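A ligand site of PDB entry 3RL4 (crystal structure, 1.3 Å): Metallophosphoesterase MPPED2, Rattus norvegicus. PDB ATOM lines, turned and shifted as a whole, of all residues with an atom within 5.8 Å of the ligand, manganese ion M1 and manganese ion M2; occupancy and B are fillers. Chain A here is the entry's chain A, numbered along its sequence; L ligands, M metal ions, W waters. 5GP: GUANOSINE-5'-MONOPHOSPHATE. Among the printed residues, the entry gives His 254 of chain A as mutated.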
ATOM      1  N   ASP A  67       8.257 -31.383 -21.021  1.00  0.00           N
ATOM      2  CA  ASP A  67       7.361 -32.302 -21.725  1.00  0.00           C
ATOM      3  C   ASP A  67       8.007 -33.676 -21.820  1.00  0.00           C
ATOM      4  O   ASP A  67       8.018 -34.320 -22.880  1.00  0.00           O
ATOM      5  CB  ASP A  67       7.015 -31.746 -23.112  1.00  0.00           C
ATOM      6  CG  ASP A  67       6.211 -30.473 -22.995  1.00  0.00           C
ATOM      7  OD1 ASP A  67       4.979 -30.576 -22.874  1.00  0.00           O
ATOM      8  OD2 ASP A  67       6.820 -29.384 -22.971  1.00  0.00           O
ATOM      9  N   HIS A  69       6.795 -36.107 -19.923  1.00  0.00           N
ATOM     10  CA  HIS A  69       5.577 -36.934 -19.966  1.00  0.00           C
ATOM     11  C   HIS A  69       5.799 -38.337 -19.391  1.00  0.00           C
ATOM     12  O   HIS A  69       5.263 -39.319 -19.909  1.00  0.00           O
ATOM     13  CB  HIS A  69       4.977 -36.959 -21.386  1.00  0.00           C
ATOM     14  CG  HIS A  69       4.291 -35.683 -21.783  1.00  0.00           C
ATOM     15  ND1 HIS A  69       3.048 -35.325 -21.296  1.00  0.00           N
ATOM     16  CD2 HIS A  69       4.692 -34.645 -22.568  1.00  0.00           C
ATOM     17  CE1 HIS A  69       2.697 -34.162 -21.797  1.00  0.00           C
ATOM     18  NE2 HIS A  69       3.676 -33.722 -22.570  1.00  0.00           N
ATOM     19  N   GLY A  87       7.707 -28.213 -17.521  1.00  0.00           N
ATOM     20  CA  GLY A  87       6.354 -28.722 -17.222  1.00  0.00           C
ATOM     21  C   GLY A  87       5.960 -29.913 -18.078  1.00  0.00           C
ATOM     22  O   GLY A  87       6.688 -30.351 -18.983  1.00  0.00           O
ATOM     23  N   ASP A  88       4.764 -30.442 -17.818  1.00  0.00           N
ATOM     24  CA  ASP A  88       4.336 -31.722 -18.420  1.00  0.00           C
ATOM     25  C   ASP A  88       5.375 -32.810 -18.102  1.00  0.00           C
ATOM     26  O   ASP A  88       5.847 -33.543 -18.998  1.00  0.00           O
ATOM     27  CB  ASP A  88       4.091 -31.615 -19.929  1.00  0.00           C
ATOM     28  CG  ASP A  88       2.717 -31.026 -20.276  1.00  0.00           C
ATOM     29  OD1 ASP A  88       1.940 -30.686 -19.350  1.00  0.00           O
ATOM     30  OD2 ASP A  88       2.464 -30.890 -21.512  1.00  0.00           O
ATOM     31  N   GLY A 118       3.007 -28.122 -16.016  1.00  0.00           N
ATOM     32  CA  GLY A 118       2.271 -27.845 -17.233  1.00  0.00           C
ATOM     33  C   GLY A 118       0.826 -28.326 -17.141  1.00  0.00           C
ATOM     34  O   GLY A 118       0.328 -28.695 -16.059  1.00  0.00           O
ATOM     35  N   ASN A 119       0.178 -28.375 -18.295  1.00  0.00           N
ATOM     36  CA  ASN A 119      -1.249 -28.679 -18.330  1.00  0.00           C
ATOM     37  C   ASN A 119      -1.587 -30.113 -17.946  1.00  0.00           C
ATOM     38  O   ASN A 119      -2.738 -30.412 -17.578  1.00  0.00           O
ATOM     39  CB  ASN A 119      -1.879 -28.270 -19.674  1.00  0.00           C
ATOM     40  CG  ASN A 119      -1.183 -28.856 -20.837  1.00  0.00           C
ATOM     41  OD1 ASN A 119       0.022 -28.633 -21.023  1.00  0.00           O
ATOM     42  ND2 ASN A 119      -1.891 -29.604 -21.653  1.00  0.00           N
ATOM     43  N   HIS A 120      -0.612 -31.027 -18.055  1.00  0.00           N
ATOM     44  CA  HIS A 120      -0.872 -32.408 -17.630  1.00  0.00           C
ATOM     45  C   HIS A 120      -0.802 -32.634 -16.136  1.00  0.00           C
ATOM     46  O   HIS A 120      -1.199 -33.702 -15.667  1.00  0.00           O
ATOM     47  CB  HIS A 120       0.047 -33.386 -18.361  1.00  0.00           C
ATOM     48  CG  HIS A 120      -0.342 -33.603 -19.781  1.00  0.00           C
ATOM     49  ND1 HIS A 120      -0.904 -34.792 -20.223  1.00  0.00           N
ATOM     50  CD2 HIS A 120      -0.328 -32.779 -20.855  1.00  0.00           C
ATOM     51  CE1 HIS A 120      -1.156 -34.706 -21.516  1.00  0.00           C
ATOM     52  NE2 HIS A 120      -0.823 -33.494 -21.924  1.00  0.00           N
ATOM     53  N   PRO A 183      -2.727 -20.612 -22.766  1.00  0.00           N
ATOM     54  CA  PRO A 183      -4.016 -20.355 -23.414  1.00  0.00           C
ATOM     55  C   PRO A 183      -4.891 -21.596 -23.437  1.00  0.00           C
ATOM     56  O   PRO A 183      -4.409 -22.684 -23.784  1.00  0.00           O
ATOM     57  CB  PRO A 183      -3.611 -19.976 -24.841  1.00  0.00           C
ATOM     58  CG  PRO A 183      -2.250 -19.357 -24.701  1.00  0.00           C
ATOM     59  CD  PRO A 183      -1.588 -20.168 -23.606  1.00  0.00           C
ATOM     60  N   TRP A 184      -6.165 -21.413 -23.120  1.00  0.00           N
ATOM     61  CA  TRP A 184      -7.144 -22.499 -23.028  1.00  0.00           C
ATOM     62  C   TRP A 184      -7.127 -23.346 -24.298  1.00  0.00           C
ATOM     63  O   TRP A 184      -7.169 -22.836 -25.421  1.00  0.00           O
ATOM     64  CB  TRP A 184      -8.540 -21.929 -22.771  1.00  0.00           C
ATOM     65  CG  TRP A 184      -9.527 -22.870 -22.057  1.00  0.00           C
ATOM     66  CD1 TRP A 184      -9.812 -22.884 -20.723  1.00  0.00           C
ATOM     67  CD2 TRP A 184     -10.347 -23.883 -22.648  1.00  0.00           C
ATOM     68  NE1 TRP A 184     -10.755 -23.854 -20.442  1.00  0.00           N
ATOM     69  CE2 TRP A 184     -11.094 -24.482 -21.604  1.00  0.00           C
ATOM     70  CE3 TRP A 184     -10.519 -24.365 -23.956  1.00  0.00           C
ATOM     71  CZ2 TRP A 184     -12.006 -25.524 -21.825  1.00  0.00           C
ATOM     72  CZ3 TRP A 184     -11.435 -25.401 -24.170  1.00  0.00           C
ATOM     73  CH2 TRP A 184     -12.154 -25.963 -23.112  1.00  0.00           C
ATOM     74  N   PHE A 185      -7.038 -24.644 -24.093  1.00  0.00           N
ATOM     75  CA  PHE A 185      -7.085 -25.582 -25.190  1.00  0.00           C
ATOM     76  C   PHE A 185      -8.196 -26.633 -24.950  1.00  0.00           C
ATOM     77  O   PHE A 185      -9.109 -26.763 -25.773  1.00  0.00           O
ATOM     78  CB  PHE A 185      -5.694 -26.196 -25.375  1.00  0.00           C
ATOM     79  CG  PHE A 185      -5.622 -27.213 -26.473  1.00  0.00           C
ATOM     80  CD1 PHE A 185      -6.020 -26.902 -27.768  1.00  0.00           C
ATOM     81  CD2 PHE A 185      -5.147 -28.493 -26.212  1.00  0.00           C
ATOM     82  CE1 PHE A 185      -5.945 -27.853 -28.792  1.00  0.00           C
ATOM     83  CE2 PHE A 185      -5.062 -29.457 -27.220  1.00  0.00           C
ATOM     84  CZ  PHE A 185      -5.466 -29.130 -28.518  1.00  0.00           C
ATOM     85  N   ASN A 186      -8.161 -27.293 -23.799  1.00  0.00           N
ATOM     86  CA  ASN A 186      -9.116 -28.390 -23.509  1.00  0.00           C
ATOM     87  C   ASN A 186      -9.560 -28.426 -22.051  1.00  0.00           C
ATOM     88  O   ASN A 186     -10.181 -29.385 -21.621  1.00  0.00           O
ATOM     89  CB  ASN A 186      -8.516 -29.748 -23.888  1.00  0.00           C
ATOM     90  CG  ASN A 186      -7.126 -29.948 -23.310  1.00  0.00           C
ATOM     91  OD1 ASN A 186      -6.711 -29.226 -22.385  1.00  0.00           O
ATOM     92  ND2 ASN A 186      -6.396 -30.918 -23.834  1.00  0.00           N
ATOM     93  N   ARG A 194      -7.506 -16.530 -23.355  1.00  0.00           N
ATOM     94  CA  ARG A 194      -6.640 -15.477 -23.837  1.00  0.00           C
ATOM     95  C   ARG A 194      -7.102 -14.100 -23.372  1.00  0.00           C
ATOM     96  O   ARG A 194      -8.295 -13.880 -23.109  1.00  0.00           O
ATOM     97  CB  ARG A 194      -6.529 -15.540 -25.368  1.00  0.00           C
ATOM     98  CG  ARG A 194      -5.765 -16.761 -25.860  1.00  0.00           C
ATOM     99  CD  ARG A 194      -5.735 -16.888 -27.401  1.00  0.00           C
ATOM    100  NE  ARG A 194      -5.161 -18.166 -27.813  1.00  0.00           N
ATOM    101  CZ  ARG A 194      -3.850 -18.401 -27.948  1.00  0.00           C
ATOM    102  NH1 ARG A 194      -2.953 -17.444 -27.711  1.00  0.00           N
ATOM    103  NH2 ARG A 194      -3.449 -19.613 -28.297  1.00  0.00           N
ATOM    104  N   HIS A 215       5.089 -22.708 -19.142  1.00  0.00           N
ATOM    105  CA  HIS A 215       4.910 -23.990 -19.774  1.00  0.00           C
ATOM    106  C   HIS A 215       4.850 -23.856 -21.288  1.00  0.00           C
ATOM    107  O   HIS A 215       5.401 -24.677 -22.021  1.00  0.00           O
ATOM    108  CB  HIS A 215       3.712 -24.768 -19.256  1.00  0.00           C
ATOM    109  CG  HIS A 215       3.523 -26.076 -19.969  1.00  0.00           C
ATOM    110  ND1 HIS A 215       4.532 -27.015 -20.082  1.00  0.00           N
ATOM    111  CD2 HIS A 215       2.454 -26.596 -20.632  1.00  0.00           C
ATOM    112  CE1 HIS A 215       4.102 -28.036 -20.800  1.00  0.00           C
ATOM    113  NE2 HIS A 215       2.849 -27.813 -21.158  1.00  0.00           N
ATOM    114  N   VAL A 225       1.732 -24.753 -34.814  1.00  0.00           N
ATOM    115  CA  VAL A 225       1.100 -26.074 -34.727  1.00  0.00           C
ATOM    116  C   VAL A 225       0.725 -26.516 -36.146  1.00  0.00           C
ATOM    117  O   VAL A 225      -0.258 -26.007 -36.702  1.00  0.00           O
ATOM    118  CB  VAL A 225      -0.141 -26.087 -33.806  1.00  0.00           C
ATOM    119  CG1 VAL A 225      -0.784 -27.483 -33.737  1.00  0.00           C
ATOM    120  CG2 VAL A 225       0.241 -25.632 -32.407  1.00  0.00           C
ATOM    121  N   GLU A 228      -3.093 -27.615 -37.199  1.00  0.00           N
ATOM    122  CA  GLU A 228      -4.102 -26.562 -37.337  1.00  0.00           C
ATOM    123  C   GLU A 228      -3.660 -25.424 -38.245  1.00  0.00           C
ATOM    124  O   GLU A 228      -4.461 -24.542 -38.552  1.00  0.00           O
ATOM    125  CB  GLU A 228      -4.523 -26.015 -35.970  1.00  0.00           C
ATOM    126  CG  GLU A 228      -5.525 -26.888 -35.207  1.00  0.00           C
ATOM    127  CD  GLU A 228      -4.869 -28.068 -34.531  1.00  0.00           C
ATOM    128  OE1 GLU A 228      -3.639 -28.044 -34.319  1.00  0.00           O
ATOM    129  OE2 GLU A 228      -5.589 -29.039 -34.198  1.00  0.00           O
ATOM    130  N   GLN A 230      -1.712 -22.973 -37.416  1.00  0.00           N
ATOM    131  CA  GLN A 230      -1.931 -21.790 -36.593  1.00  0.00           C
ATOM    132  C   GLN A 230      -0.761 -21.577 -35.642  1.00  0.00           C
ATOM    133  O   GLN A 230      -0.139 -22.527 -35.173  1.00  0.00           O
ATOM    134  CB  GLN A 230      -3.216 -21.936 -35.757  1.00  0.00           C
ATOM    135  CG  GLN A 230      -4.506 -21.865 -36.551  1.00  0.00           C
ATOM    136  CD  GLN A 230      -5.756 -21.722 -35.699  1.00  0.00           C
ATOM    137  OE1 GLN A 230      -5.722 -21.906 -34.474  1.00  0.00           O
ATOM    138  NE2 GLN A 230      -6.880 -21.395 -36.341  1.00  0.00           N
ATOM    139  N   VAL A 232       0.045 -20.460 -31.859  1.00  0.00           N
ATOM    140  CA  VAL A 232      -0.769 -20.618 -30.655  1.00  0.00           C
ATOM    141  C   VAL A 232      -0.118 -19.992 -29.421  1.00  0.00           C
ATOM    142  O   VAL A 232      -0.676 -20.103 -28.335  1.00  0.00           O
ATOM    143  CB  VAL A 232      -1.139 -22.094 -30.366  1.00  0.00           C
ATOM    144  CG1 VAL A 232      -1.864 -22.740 -31.582  1.00  0.00           C
ATOM    145  CG2 VAL A 232       0.109 -22.898 -30.004  1.00  0.00           C
ATOM    146  N   HIS A 254       5.498 -27.173 -24.243  1.00  0.00           N
ATOM    147  CA  HIS A 254       4.053 -27.277 -24.535  1.00  0.00           C
ATOM    148  C   HIS A 254       3.740 -27.629 -25.975  1.00  0.00           C
ATOM    149  O   HIS A 254       2.959 -28.556 -26.228  1.00  0.00           O
ATOM    150  CB  HIS A 254       3.310 -26.025 -24.056  1.00  0.00           C
ATOM    151  CG  HIS A 254       1.818 -26.117 -24.150  1.00  0.00           C
ATOM    152  ND1 HIS A 254       1.081 -27.157 -23.610  1.00  0.00           N
ATOM    153  CD2 HIS A 254       0.929 -25.268 -24.711  1.00  0.00           C
ATOM    154  CE1 HIS A 254      -0.205 -26.921 -23.804  1.00  0.00           C
ATOM    155  NE2 HIS A 254      -0.322 -25.782 -24.477  1.00  0.00           N
ATOM    156  N   ILE A 255       4.281 -26.827 -26.889  1.00  0.00           N
ATOM    157  CA  ILE A 255       4.135 -27.119 -28.314  1.00  0.00           C
ATOM    158  C   ILE A 255       5.314 -27.967 -28.733  1.00  0.00           C
ATOM    159  O   ILE A 255       6.399 -27.439 -29.052  1.00  0.00           O
ATOM    160  CB  ILE A 255       3.993 -25.821 -29.135  1.00  0.00           C
ATOM    161  CG1 ILE A 255       2.829 -24.960 -28.595  1.00  0.00           C
ATOM    162  CG2 ILE A 255       3.844 -26.143 -30.635  1.00  0.00           C
ATOM    163  CD1 ILE A 255       1.488 -25.689 -28.409  1.00  0.00           C
ATOM    164  N   HIS A 256       5.113 -29.281 -28.669  1.00  0.00           N
ATOM    165  CA  HIS A 256       6.245 -30.214 -28.817  1.00  0.00           C
ATOM    166  C   HIS A 256       6.968 -30.018 -30.140  1.00  0.00           C
ATOM    167  O   HIS A 256       8.210 -30.103 -30.207  1.00  0.00           O
ATOM    168  CB  HIS A 256       5.750 -31.654 -28.704  1.00  0.00           C
ATOM    169  CG  HIS A 256       5.169 -32.030 -27.372  1.00  0.00           C
ATOM    170  ND1 HIS A 256       4.738 -33.318 -27.123  1.00  0.00           N
ATOM    171  CD2 HIS A 256       4.910 -31.318 -26.237  1.00  0.00           C
ATOM    172  CE1 HIS A 256       4.250 -33.391 -25.892  1.00  0.00           C
ATOM    173  NE2 HIS A 256       4.340 -32.195 -25.337  1.00  0.00           N
ATOM    174  N   GLU A 257       6.191 -29.717 -31.179  1.00  0.00           N
ATOM    175  CA  GLU A 257       6.660 -29.538 -32.555  1.00  0.00           C
ATOM    176  C   GLU A 257       7.647 -28.388 -32.664  1.00  0.00           C
ATOM    177  O   GLU A 257       8.426 -28.320 -33.614  1.00  0.00           O
ATOM    178  CB  GLU A 257       5.493 -29.246 -33.508  1.00  0.00           C
ATOM    179  CG  GLU A 257       4.335 -30.248 -33.535  1.00  0.00           C
ATOM    180  CD  GLU A 257       3.237 -29.847 -32.581  1.00  0.00           C
ATOM    181  OE1 GLU A 257       3.497 -29.810 -31.377  1.00  0.00           O
ATOM    182  OE2 GLU A 257       2.084 -29.619 -33.012  1.00  0.00           O
ATOM    183  N   THR A 276       8.320 -35.493 -28.844  1.00  0.00           N
ATOM    184  CA  THR A 276       7.771 -35.020 -30.112  1.00  0.00           C
ATOM    185  C   THR A 276       6.227 -34.959 -30.009  1.00  0.00           C
ATOM    186  O   THR A 276       5.630 -35.323 -28.983  1.00  0.00           O
ATOM    187  CB  THR A 276       8.117 -36.019 -31.214  1.00  0.00           C
ATOM    188  OG1 THR A 276       7.512 -37.269 -30.881  1.00  0.00           O
ATOM    189  CG2 THR A 276       9.636 -36.168 -31.358  1.00  0.00           C
ATOM    190  N   VAL A 277       5.574 -34.495 -31.066  1.00  0.00           N
ATOM    191  CA  VAL A 277       4.117 -34.452 -31.080  1.00  0.00           C
ATOM    192  C   VAL A 277       3.463 -35.845 -30.896  1.00  0.00           C
ATOM    193  O   VAL A 277       2.311 -35.949 -30.459  1.00  0.00           O
ATOM    194  CB  VAL A 277       3.581 -33.698 -32.324  1.00  0.00           C
ATOM    195  CG1 VAL A 277       3.821 -34.502 -33.590  1.00  0.00           C
ATOM    196  CG2 VAL A 277       2.086 -33.299 -32.152  1.00  0.00           C
ATOM    197  N   PHE A 279       4.724 -37.960 -28.774  1.00  0.00           N
ATOM    198  CA  PHE A 279       5.077 -38.321 -27.395  1.00  0.00           C
ATOM    199  C   PHE A 279       6.285 -39.284 -27.302  1.00  0.00           C
ATOM    200  O   PHE A 279       6.376 -40.097 -26.373  1.00  0.00           O
ATOM    201  CB  PHE A 279       3.839 -38.821 -26.605  1.00  0.00           C
ATOM    202  CG  PHE A 279       2.910 -37.717 -26.140  1.00  0.00           C
ATOM    203  CD1 PHE A 279       2.122 -37.001 -27.051  1.00  0.00           C
ATOM    204  CD2 PHE A 279       2.815 -37.383 -24.793  1.00  0.00           C
ATOM    205  CE1 PHE A 279       1.264 -35.978 -26.608  1.00  0.00           C
ATOM    206  CE2 PHE A 279       1.955 -36.373 -24.354  1.00  0.00           C
ATOM    207  CZ  PHE A 279       1.193 -35.671 -25.255  1.00  0.00           C
HETATM  208  P   5GP L   1       0.167 -31.376 -24.328  1.00  0.00           P
HETATM  209  O1P 5GP L   1      -0.006 -30.195 -23.464  1.00  0.00           O
HETATM  210  O2P 5GP L   1       1.401 -32.341 -23.919  1.00  0.00           O
HETATM  211  O3P 5GP L   1      -1.102 -32.290 -24.262  1.00  0.00           O
HETATM  212  O5' 5GP L   1       0.382 -30.919 -25.847  1.00  0.00           O
HETATM  213  C5' 5GP L   1       0.575 -31.896 -26.897  1.00  0.00           C
HETATM  214  C4' 5GP L   1       0.338 -31.277 -28.261  1.00  0.00           C
HETATM  215  O4' 5GP L   1      -0.988 -30.727 -28.251  1.00  0.00           O
HETATM  216  C3' 5GP L   1       1.195 -30.062 -28.610  1.00  0.00           C
HETATM  217  O3' 5GP L   1       2.511 -30.473 -29.045  1.00  0.00           O
HETATM  218  C2' 5GP L   1       0.367 -29.442 -29.729  1.00  0.00           C
HETATM  219  O2' 5GP L   1       0.490 -30.198 -30.944  1.00  0.00           O
HETATM  220  C1' 5GP L   1      -1.063 -29.647 -29.185  1.00  0.00           C
HETATM  221  N9  5GP L   1      -1.499 -28.406 -28.480  1.00  0.00           N
HETATM  222  C8  5GP L   1      -1.228 -28.009 -27.218  1.00  0.00           C
HETATM  223  N7  5GP L   1      -1.803 -26.836 -27.000  1.00  0.00           N
HETATM  224  C5  5GP L   1      -2.431 -26.461 -28.111  1.00  0.00           C
HETATM  225  C6  5GP L   1      -3.176 -25.346 -28.471  1.00  0.00           C
HETATM  226  O6  5GP L   1      -3.402 -24.408 -27.696  1.00  0.00           O
HETATM  227  N1  5GP L   1      -3.705 -25.296 -29.747  1.00  0.00           N
HETATM  228  C2  5GP L   1      -3.470 -26.334 -30.660  1.00  0.00           C
HETATM  229  N2  5GP L   1      -3.995 -26.250 -31.877  1.00  0.00           N
HETATM  230  N3  5GP L   1      -2.753 -27.403 -30.295  1.00  0.00           N
HETATM  231  C4  5GP L   1      -2.233 -27.473 -29.050  1.00  0.00           C
HETATM  232 MN    MN M   1       3.357 -31.745 -23.389  1.00  0.00          MN
HETATM  233 MN    MN M   2       1.532 -29.054 -22.439  1.00  0.00          MN
HETATM  234  O   HOH W   1      -1.259 -31.182 -32.802  1.00  0.00           O
HETATM  235  O   HOH W   2      -5.782 -23.805 -30.815  1.00  0.00           O
HETATM  236  O   HOH W   3      -5.182 -22.293 -27.867  1.00  0.00           O
HETATM  237  O   HOH W   4      -2.052 -23.494 -25.450  1.00  0.00           O
HETATM  238  O   HOH W   5       2.578 -29.870 -23.842  1.00  0.00           O
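Merely in contact with the ligand: Phe 185 (3.3 Å), Val 225 (3.9 Å), Val 232 (3.6 Å), Ile 255 (3.8 Å), Val 277 (3.7 Å) and Phe 279 (3.6 Å).
Hydrophobic or aromatic side chains that line the ligand: His 69, His 120, Phe 185, Val 225, Val 232, His 254, Ile 255, His 256, Val 277 and Phe 279.
14 residues have an atom within 4 Å of the ligand: His 69, Asp 88, Asn 119, His 120, Phe 185, Val 225, Glu 228, Val 232, His 254, Ile 255, His 256, Glu 257, Val 277 and Phe 279.
The nearest printed residue that does not touch the ligand is Asp 67 (4.1 Å).
Water W5 bridges O of His 254 (2.8 Å) and O5' of the ligand (3.2 Å).
Water W3 lies within hydrogen-bond range of O6 of the ligand, O of Trp 184 and NH2 of Arg 194.
Water W4 lies within hydrogen-bond range of an oxygen (O6) of the ligand, the backbone carbonyl oxygen (O) of Pro 183 and a ring nitrogen (NE2) of His 254.
Five residues have an atom within 4 Å of manganese ion M2: Asp 67, Asp 88, Asn 119, His 215 and His 254.
The nearest printed residue that does not touch manganese ion M2 is His 120 (4.5 Å).
The backbone carbonyl oxygen (O) of Val 232 lies within hydrogen-bond range of the guanidinium group (NH2) of Arg 194.
A ring nitrogen (ND1) of His 256 lies within hydrogen-bond range of the backbone carbonyl oxygen (O) of Thr 276, 2.9 Å away.
The backbone NH (N) of Val 225 sits at hydrogen-bond distance from the backbone carbonyl oxygen (O) of Gln 230 (2.9 Å).
The side-chain carboxylate (OD2) of Asp 67 lies within hydrogen-bond range of the backbone NH (N) of His 254, 2.9 Å away.
The side-chain carboxylate of Asp 88 lies within hydrogen-bond range of the backbone NH of His 120.
The backbone NH (N) of Asp 67 is in hydrogen-bond range of the backbone carbonyl oxygen (O) of Gly 87, at 2.8 Å.
OD1 of Asp 67 binds manganese ion M1 (2.1 Å).
Water W5 binds manganese ion M1, 2.1 Å away.
Manganese ion M1 is bound by an oxygen (O2P) of the ligand.
Manganese ion M1 is bound by NE2 of His 69.
Manganese ion M1 is bound by NE2 of His 256, at 2.2 Å.
OD2 of Asp 88 is bound to manganese ion M1.
Manganese ion M1 has six donor atoms within binding distance.
The side-chain carboxylate of Glu 228 sits at hydrogen-bond distance from a nitrogen (N2) of the ligand, 3.1 Å away.
O of His 254 sits close to O3' of the ligand (3.4 Å).
A ring nitrogen (NE2) of His 120 is in hydrogen-bond range of an oxygen (O3P) of the ligand (2.6 Å).
OE1 of Glu 257 lies within hydrogen-bond range of O3' of the ligand (2.6 Å).
The backbone NH (N) of His 256 is in hydrogen-bond range of an oxygen (O3') of the ligand (2.9 Å).
Manganese ion M2 is bound by water W5 (1.9 Å), OD1 of Asn 119 (2.1 Å), O1P of the ligand (2.2 Å), NE2 of His 215 (2.2 Å), OD2 of Asp 88 (2.3 Å) and ND1 of His 254 (2.3 Å).
Manganese ion M2 has six donor atoms within binding distance.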
